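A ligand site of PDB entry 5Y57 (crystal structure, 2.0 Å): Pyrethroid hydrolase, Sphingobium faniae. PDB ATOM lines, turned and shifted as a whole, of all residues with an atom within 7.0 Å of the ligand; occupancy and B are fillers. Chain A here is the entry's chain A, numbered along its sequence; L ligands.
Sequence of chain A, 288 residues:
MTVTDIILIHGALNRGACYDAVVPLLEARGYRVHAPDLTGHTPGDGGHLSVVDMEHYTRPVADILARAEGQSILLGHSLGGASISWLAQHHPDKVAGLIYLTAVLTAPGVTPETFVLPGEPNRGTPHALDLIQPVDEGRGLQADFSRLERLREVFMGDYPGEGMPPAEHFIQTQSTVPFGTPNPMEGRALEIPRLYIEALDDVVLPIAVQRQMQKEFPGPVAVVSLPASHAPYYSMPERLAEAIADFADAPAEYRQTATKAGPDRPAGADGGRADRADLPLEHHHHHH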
ATOM      1  N   HIS A  10     -17.276 -30.621  20.985  1.00  0.00           N
ATOM      2  CA  HIS A  10     -16.745 -29.991  22.179  1.00  0.00           C
ATOM      3  C   HIS A  10     -16.853 -28.459  22.101  1.00  0.00           C
ATOM      4  O   HIS A  10     -17.013 -27.861  21.042  1.00  0.00           O
ATOM      5  CB  HIS A  10     -15.283 -30.397  22.360  1.00  0.00           C
ATOM      6  CG  HIS A  10     -14.404 -29.976  21.210  1.00  0.00           C
ATOM      7  ND1 HIS A  10     -14.060 -28.665  20.985  1.00  0.00           N
ATOM      8  CD2 HIS A  10     -13.854 -30.691  20.206  1.00  0.00           C
ATOM      9  CE1 HIS A  10     -13.307 -28.595  19.889  1.00  0.00           C
ATOM     10  NE2 HIS A  10     -13.178 -29.816  19.403  1.00  0.00           N
ATOM     11  N   GLY A  11     -16.715 -27.827  23.260  1.00  0.00           N
ATOM     12  CA  GLY A  11     -16.665 -26.381  23.357  1.00  0.00           C
ATOM     13  C   GLY A  11     -15.226 -25.857  23.337  1.00  0.00           C
ATOM     14  O   GLY A  11     -14.277 -26.572  23.015  1.00  0.00           O
ATOM     15  N   ALA A  12     -15.074 -24.577  23.690  1.00  0.00           N
ATOM     16  CA  ALA A  12     -13.765 -23.938  23.612  1.00  0.00           C
ATOM     17  C   ALA A  12     -12.734 -24.591  24.540  1.00  0.00           C
ATOM     18  O   ALA A  12     -13.039 -24.999  25.666  1.00  0.00           O
ATOM     19  CB  ALA A  12     -13.902 -22.452  23.942  1.00  0.00           C
ATOM     20  N   LEU A  13     -11.504 -24.665  24.057  1.00  0.00           N
ATOM     21  CA  LEU A  13     -10.360 -25.218  24.789  1.00  0.00           C
ATOM     22  C   LEU A  13     -10.510 -26.718  25.127  1.00  0.00           C
ATOM     23  O   LEU A  13      -9.685 -27.259  25.870  1.00  0.00           O
ATOM     24  CB  LEU A  13     -10.089 -24.429  26.069  1.00  0.00           C
ATOM     25  CG  LEU A  13      -9.633 -22.972  25.860  1.00  0.00           C
ATOM     26  CD1 LEU A  13      -9.897 -22.116  27.097  1.00  0.00           C
ATOM     27  CD2 LEU A  13      -8.182 -22.971  25.517  1.00  0.00           C
ATOM     28  N   ASN A  14     -11.520 -27.397  24.615  1.00  0.00           N
ATOM     29  CA  ASN A  14     -11.742 -28.811  24.902  1.00  0.00           C
ATOM     30  C   ASN A  14     -11.466 -29.660  23.664  1.00  0.00           C
ATOM     31  O   ASN A  14     -11.243 -29.140  22.569  1.00  0.00           O
ATOM     32  CB  ASN A  14     -13.190 -29.037  25.381  1.00  0.00           C
ATOM     33  CG  ASN A  14     -13.354 -28.780  26.860  1.00  0.00           C
ATOM     34  OD1 ASN A  14     -13.062 -27.692  27.363  1.00  0.00           O
ATOM     35  ND2 ASN A  14     -13.838 -29.796  27.580  1.00  0.00           N
ATOM     36  N   HIS A  77     -21.635 -28.311  22.608  1.00  0.00           N
ATOM     37  CA  HIS A  77     -21.531 -27.874  23.999  1.00  0.00           C
ATOM     38  C   HIS A  77     -20.867 -26.497  24.056  1.00  0.00           C
ATOM     39  O   HIS A  77     -19.837 -26.271  23.408  1.00  0.00           O
ATOM     40  CB  HIS A  77     -20.752 -28.865  24.854  1.00  0.00           C
ATOM     41  CG  HIS A  77     -20.403 -28.342  26.218  1.00  0.00           C
ATOM     42  ND1 HIS A  77     -19.111 -27.967  26.550  1.00  0.00           N
ATOM     43  CD2 HIS A  77     -21.153 -28.106  27.324  1.00  0.00           C
ATOM     44  CE1 HIS A  77     -19.080 -27.552  27.809  1.00  0.00           C
ATOM     45  NE2 HIS A  77     -20.318 -27.591  28.282  1.00  0.00           N
ATOM     46  N   SER A  78     -21.386 -25.614  24.904  1.00  0.00           N
ATOM     47  CA  SER A  78     -20.756 -24.318  25.161  1.00  0.00           C
ATOM     48  C   SER A  78     -20.593 -23.624  23.808  1.00  0.00           C
ATOM     49  O   SER A  78     -21.593 -23.488  23.090  1.00  0.00           O
ATOM     50  CB  SER A  78     -19.445 -24.557  25.939  1.00  0.00           C
ATOM     51  OG  SER A  78     -18.937 -23.414  26.577  1.00  0.00           O
ATOM     52  N   LEU A  79     -19.391 -23.259  23.396  1.00  0.00           N
ATOM     53  CA  LEU A  79     -19.176 -22.616  22.106  1.00  0.00           C
ATOM     54  C   LEU A  79     -19.419 -23.545  20.930  1.00  0.00           C
ATOM     55  O   LEU A  79     -19.441 -23.081  19.776  1.00  0.00           O
ATOM     56  CB  LEU A  79     -17.751 -22.064  22.032  1.00  0.00           C
ATOM     57  CG  LEU A  79     -17.381 -21.147  20.881  1.00  0.00           C
ATOM     58  CD1 LEU A  79     -17.891 -19.780  21.213  1.00  0.00           C
ATOM     59  CD2 LEU A  79     -15.869 -21.190  20.696  1.00  0.00           C
ATOM     60  N   GLY A  80     -19.596 -24.838  21.193  1.00  0.00           N
ATOM     61  CA  GLY A  80     -19.854 -25.792  20.138  1.00  0.00           C
ATOM     62  C   GLY A  80     -21.121 -25.519  19.385  1.00  0.00           C
ATOM     63  O   GLY A  80     -21.233 -25.913  18.226  1.00  0.00           O
ATOM     64  N   THR A 102     -26.055 -26.546  27.115  1.00  0.00           N
ATOM     65  CA  THR A 102     -25.653 -25.243  27.654  1.00  0.00           C
ATOM     66  C   THR A 102     -24.719 -24.548  26.676  1.00  0.00           C
ATOM     67  O   THR A 102     -23.534 -24.254  26.936  1.00  0.00           O
ATOM     68  CB  THR A 102     -25.123 -25.374  29.088  1.00  0.00           C
ATOM     69  OG1 THR A 102     -24.983 -24.075  29.688  1.00  0.00           O
ATOM     70  CG2 THR A 102     -23.785 -26.180  29.174  1.00  0.00           C
ATOM     71  N   VAL A 104     -24.138 -22.037  22.941  1.00  0.00           N
ATOM     72  CA  VAL A 104     -24.440 -20.742  22.351  1.00  0.00           C
ATOM     73  C   VAL A 104     -25.444 -20.956  21.224  1.00  0.00           C
ATOM     74  O   VAL A 104     -25.130 -21.544  20.190  1.00  0.00           O
ATOM     75  CB  VAL A 104     -23.172 -20.035  21.858  1.00  0.00           C
ATOM     76  CG1 VAL A 104     -23.522 -18.677  21.323  1.00  0.00           C
ATOM     77  CG2 VAL A 104     -22.212 -19.889  23.003  1.00  0.00           C
ATOM     78  N   VAL A 116     -21.671 -13.441  25.195  1.00  0.00           N
ATOM     79  CA  VAL A 116     -20.496 -13.577  26.060  1.00  0.00           C
ATOM     80  C   VAL A 116     -20.139 -12.231  26.698  1.00  0.00           C
ATOM     81  O   VAL A 116     -19.863 -12.149  27.898  1.00  0.00           O
ATOM     82  CB  VAL A 116     -19.324 -14.150  25.238  1.00  0.00           C
ATOM     83  CG1 VAL A 116     -17.957 -13.900  25.913  1.00  0.00           C
ATOM     84  CG2 VAL A 116     -19.538 -15.654  24.956  1.00  0.00           C
ATOM     85  N   THR A 125     -20.893 -13.525  29.964  1.00  0.00           N
ATOM     86  CA  THR A 125     -20.321 -14.682  30.642  1.00  0.00           C
ATOM     87  C   THR A 125     -19.048 -14.244  31.359  1.00  0.00           C
ATOM     88  O   THR A 125     -17.935 -14.615  30.966  1.00  0.00           O
ATOM     89  CB  THR A 125     -20.034 -15.806  29.652  1.00  0.00           C
ATOM     90  OG1 THR A 125     -19.084 -15.365  28.687  1.00  0.00           O
ATOM     91  CG2 THR A 125     -21.320 -16.191  28.909  1.00  0.00           C
ATOM     92  N   ALA A 128     -16.220 -16.527  32.634  1.00  0.00           N
ATOM     93  CA  ALA A 128     -15.352 -17.054  31.580  1.00  0.00           C
ATOM     94  C   ALA A 128     -14.370 -15.994  31.115  1.00  0.00           C
ATOM     95  O   ALA A 128     -13.186 -16.277  30.935  1.00  0.00           O
ATOM     96  CB  ALA A 128     -16.166 -17.562  30.392  1.00  0.00           C
ATOM     97  N   LEU A 129     -14.860 -14.768  30.895  1.00  0.00           N
ATOM     98  CA  LEU A 129     -13.980 -13.714  30.398  1.00  0.00           C
ATOM     99  C   LEU A 129     -12.860 -13.424  31.375  1.00  0.00           C
ATOM    100  O   LEU A 129     -11.754 -13.063  30.964  1.00  0.00           O
ATOM    101  CB  LEU A 129     -14.770 -12.433  30.125  1.00  0.00           C
ATOM    102  CG  LEU A 129     -15.544 -12.409  28.806  1.00  0.00           C
ATOM    103  CD1 LEU A 129     -16.447 -11.214  28.763  1.00  0.00           C
ATOM    104  CD2 LEU A 129     -14.570 -12.337  27.663  1.00  0.00           C
ATOM    105  N   ILE A 132     -10.419 -16.778  31.172  1.00  0.00           N
ATOM    106  CA  ILE A 132      -9.923 -17.010  29.816  1.00  0.00           C
ATOM    107  C   ILE A 132      -9.341 -15.684  29.336  1.00  0.00           C
ATOM    108  O   ILE A 132      -9.975 -14.640  29.470  1.00  0.00           O
ATOM    109  CB  ILE A 132     -11.052 -17.514  28.896  1.00  0.00           C
ATOM    110  CG1 ILE A 132     -11.854 -18.643  29.571  1.00  0.00           C
ATOM    111  CG2 ILE A 132     -10.524 -17.988  27.575  1.00  0.00           C
ATOM    112  CD1 ILE A 132     -11.078 -19.915  29.817  1.00  0.00           C
ATOM    113  N   LEU A 141      -7.235 -17.475  22.607  1.00  0.00           N
ATOM    114  CA  LEU A 141      -7.690 -17.442  23.987  1.00  0.00           C
ATOM    115  C   LEU A 141      -7.034 -18.593  24.719  1.00  0.00           C
ATOM    116  O   LEU A 141      -6.877 -19.688  24.160  1.00  0.00           O
ATOM    117  CB  LEU A 141      -9.212 -17.559  24.098  1.00  0.00           C
ATOM    118  CG  LEU A 141     -10.048 -16.484  23.450  1.00  0.00           C
ATOM    119  CD1 LEU A 141     -11.500 -16.904  23.543  1.00  0.00           C
ATOM    120  CD2 LEU A 141      -9.823 -15.141  24.167  1.00  0.00           C
ATOM    121  N   PHE A 155     -15.181 -24.378  35.764  1.00  0.00           N
ATOM    122  CA  PHE A 155     -15.339 -25.111  34.517  1.00  0.00           C
ATOM    123  C   PHE A 155     -15.524 -26.623  34.678  1.00  0.00           C
ATOM    124  O   PHE A 155     -16.164 -27.227  33.818  1.00  0.00           O
ATOM    125  CB  PHE A 155     -14.139 -24.853  33.617  1.00  0.00           C
ATOM    126  CG  PHE A 155     -14.222 -23.561  32.864  1.00  0.00           C
ATOM    127  CD1 PHE A 155     -14.891 -23.485  31.651  1.00  0.00           C
ATOM    128  CD2 PHE A 155     -13.654 -22.388  33.399  1.00  0.00           C
ATOM    129  CE1 PHE A 155     -14.983 -22.280  30.959  1.00  0.00           C
ATOM    130  CE2 PHE A 155     -13.737 -21.183  32.695  1.00  0.00           C
ATOM    131  CZ  PHE A 155     -14.410 -21.129  31.487  1.00  0.00           C
ATOM    132  N   GLN A 174      -7.183 -21.532  21.979  1.00  0.00           N
ATOM    133  CA  GLN A 174      -8.427 -21.593  21.216  1.00  0.00           C
ATOM    134  C   GLN A 174      -8.445 -20.493  20.162  1.00  0.00           C
ATOM    135  O   GLN A 174      -8.029 -19.366  20.442  1.00  0.00           O
ATOM    136  CB  GLN A 174      -9.611 -21.417  22.149  1.00  0.00           C
ATOM    137  CG  GLN A 174     -10.952 -21.130  21.430  1.00  0.00           C
ATOM    138  CD  GLN A 174     -11.553 -22.383  20.826  1.00  0.00           C
ATOM    139  OE1 GLN A 174     -11.472 -23.463  21.407  1.00  0.00           O
ATOM    140  NE2 GLN A 174     -12.149 -22.252  19.650  1.00  0.00           N
ATOM    141  N   PHE A 179     -16.117 -17.386  17.802  1.00  0.00           N
ATOM    142  CA  PHE A 179     -16.730 -16.337  18.602  1.00  0.00           C
ATOM    143  C   PHE A 179     -17.268 -15.213  17.754  1.00  0.00           C
ATOM    144  O   PHE A 179     -18.134 -14.468  18.210  1.00  0.00           O
ATOM    145  CB  PHE A 179     -15.738 -15.757  19.591  1.00  0.00           C
ATOM    146  CG  PHE A 179     -15.523 -16.587  20.798  1.00  0.00           C
ATOM    147  CD1 PHE A 179     -16.319 -16.427  21.921  1.00  0.00           C
ATOM    148  CD2 PHE A 179     -14.494 -17.518  20.836  1.00  0.00           C
ATOM    149  CE1 PHE A 179     -16.109 -17.173  23.048  1.00  0.00           C
ATOM    150  CE2 PHE A 179     -14.266 -18.266  21.950  1.00  0.00           C
ATOM    151  CZ  PHE A 179     -15.064 -18.103  23.063  1.00  0.00           C
ATOM    152  N   VAL A 204     -20.350 -20.611  34.272  1.00  0.00           N
ATOM    153  CA  VAL A 204     -19.789 -20.129  33.020  1.00  0.00           C
ATOM    154  C   VAL A 204     -20.871 -19.464  32.196  1.00  0.00           C
ATOM    155  O   VAL A 204     -20.819 -18.265  31.892  1.00  0.00           O
ATOM    156  CB  VAL A 204     -19.136 -21.292  32.246  1.00  0.00           C
ATOM    157  CG1 VAL A 204     -18.447 -20.818  30.966  1.00  0.00           C
ATOM    158  CG2 VAL A 204     -18.174 -22.051  33.163  1.00  0.00           C
ATOM    159  N   LEU A 205     -21.900 -20.248  31.835  1.00  0.00           N
ATOM    160  CA  LEU A 205     -23.041 -19.780  31.057  1.00  0.00           C
ATOM    161  C   LEU A 205     -24.258 -19.786  31.987  1.00  0.00           C
ATOM    162  O   LEU A 205     -24.929 -20.824  32.128  1.00  0.00           O
ATOM    163  CB  LEU A 205     -23.253 -20.678  29.845  1.00  0.00           C
ATOM    164  CG  LEU A 205     -24.333 -20.205  28.885  1.00  0.00           C
ATOM    165  CD1 LEU A 205     -24.054 -18.769  28.482  1.00  0.00           C
ATOM    166  CD2 LEU A 205     -24.383 -21.143  27.694  1.00  0.00           C
ATOM    167  N   HIS A 230     -21.457 -26.676  34.539  1.00  0.00           N
ATOM    168  CA  HIS A 230     -21.061 -26.396  33.169  1.00  0.00           C
ATOM    169  C   HIS A 230     -20.798 -27.657  32.332  1.00  0.00           C
ATOM    170  O   HIS A 230     -20.899 -27.601  31.107  1.00  0.00           O
ATOM    171  CB  HIS A 230     -19.813 -25.502  33.168  1.00  0.00           C
ATOM    172  CG  HIS A 230     -19.364 -25.130  31.796  1.00  0.00           C
ATOM    173  ND1 HIS A 230     -20.096 -24.281  30.990  1.00  0.00           N
ATOM    174  CD2 HIS A 230     -18.302 -25.534  31.065  1.00  0.00           C
ATOM    175  CE1 HIS A 230     -19.476 -24.148  29.834  1.00  0.00           C
ATOM    176  NE2 HIS A 230     -18.401 -24.903  29.841  1.00  0.00           N
HETATM  177  C1  LIG L   1     -18.061 -21.194  26.693  1.00  0.00           C
HETATM  178  S1  LIG L   1     -17.533 -22.747  26.359  1.00  0.00           S
HETATM  179  C2  LIG L   1     -17.042 -20.078  26.749  1.00  0.00           C
HETATM  180  C3  LIG L   1     -15.705 -20.328  27.009  1.00  0.00           C
HETATM  181  C4  LIG L   1     -14.794 -19.264  27.054  1.00  0.00           C
HETATM  182  C5  LIG L   1     -15.245 -17.979  26.856  1.00  0.00           C
HETATM  183  C6  LIG L   1     -16.582 -17.729  26.596  1.00  0.00           C
HETATM  184  C7  LIG L   1     -17.487 -18.775  26.555  1.00  0.00           C
HETATM  185  O1  LIG L   1     -17.099 -22.987  25.019  1.00  0.00           O
HETATM  186  O2  LIG L   1     -16.613 -23.309  27.304  1.00  0.00           O
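A sulfur (S1) of the ligand is covalently linked to the side-chain hydroxyl (OG) of Ser 78, 1.6 Å away.
N of Leu 79 sits at hydrogen-bond distance from O1 of the ligand.
The backbone NH (N) of Ala 12 sits at hydrogen-bond distance from an oxygen (O1) of the ligand (2.9 Å).
O2 of the ligand sits at hydrogen-bond distance from NE2 of His 230 (3.5 Å).
CA of Gly 11 touches O1 of the ligand (3.8 Å).
Val 116 touches the ligand (CG2 to C6, 3.97 Å).
CB of Ala 128 touches C5 of the ligand, at 3.7 Å.
Ile 132 touches the ligand.
CE1 of Phe 179 touches C6 of the ligand, 3.6 Å away.
Hydrophobic or aromatic side chains that line the ligand: Ala 12, Leu 79, Val 116, Ala 128, Ile 132, Phe 179 and His 230.
Of the 23 residues printed, 9 come within 4 Å of the ligand.
O of Ser 78 lies within hydrogen-bond range of N of Val 104.
The backbone carbonyl oxygen of Thr 102 sits at hydrogen-bond distance from the backbone NH of Ser 78 (3.3 Å).
The backbone carbonyl oxygen of Ala 12 lies close to the side-chain amide oxygen of Asn 14, at 3.2 Å.
The backbone carbonyl oxygen of His 230 is in hydrogen-bond range of a ring nitrogen (NE2) of His 77, at 2.9 Å.
The backbone NH of Gly 11 lies close to the backbone carbonyl oxygen of His 77 (3.5 Å).
O of Val 116 lies within hydrogen-bond range of N of Thr 125, at 2.7 Å.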
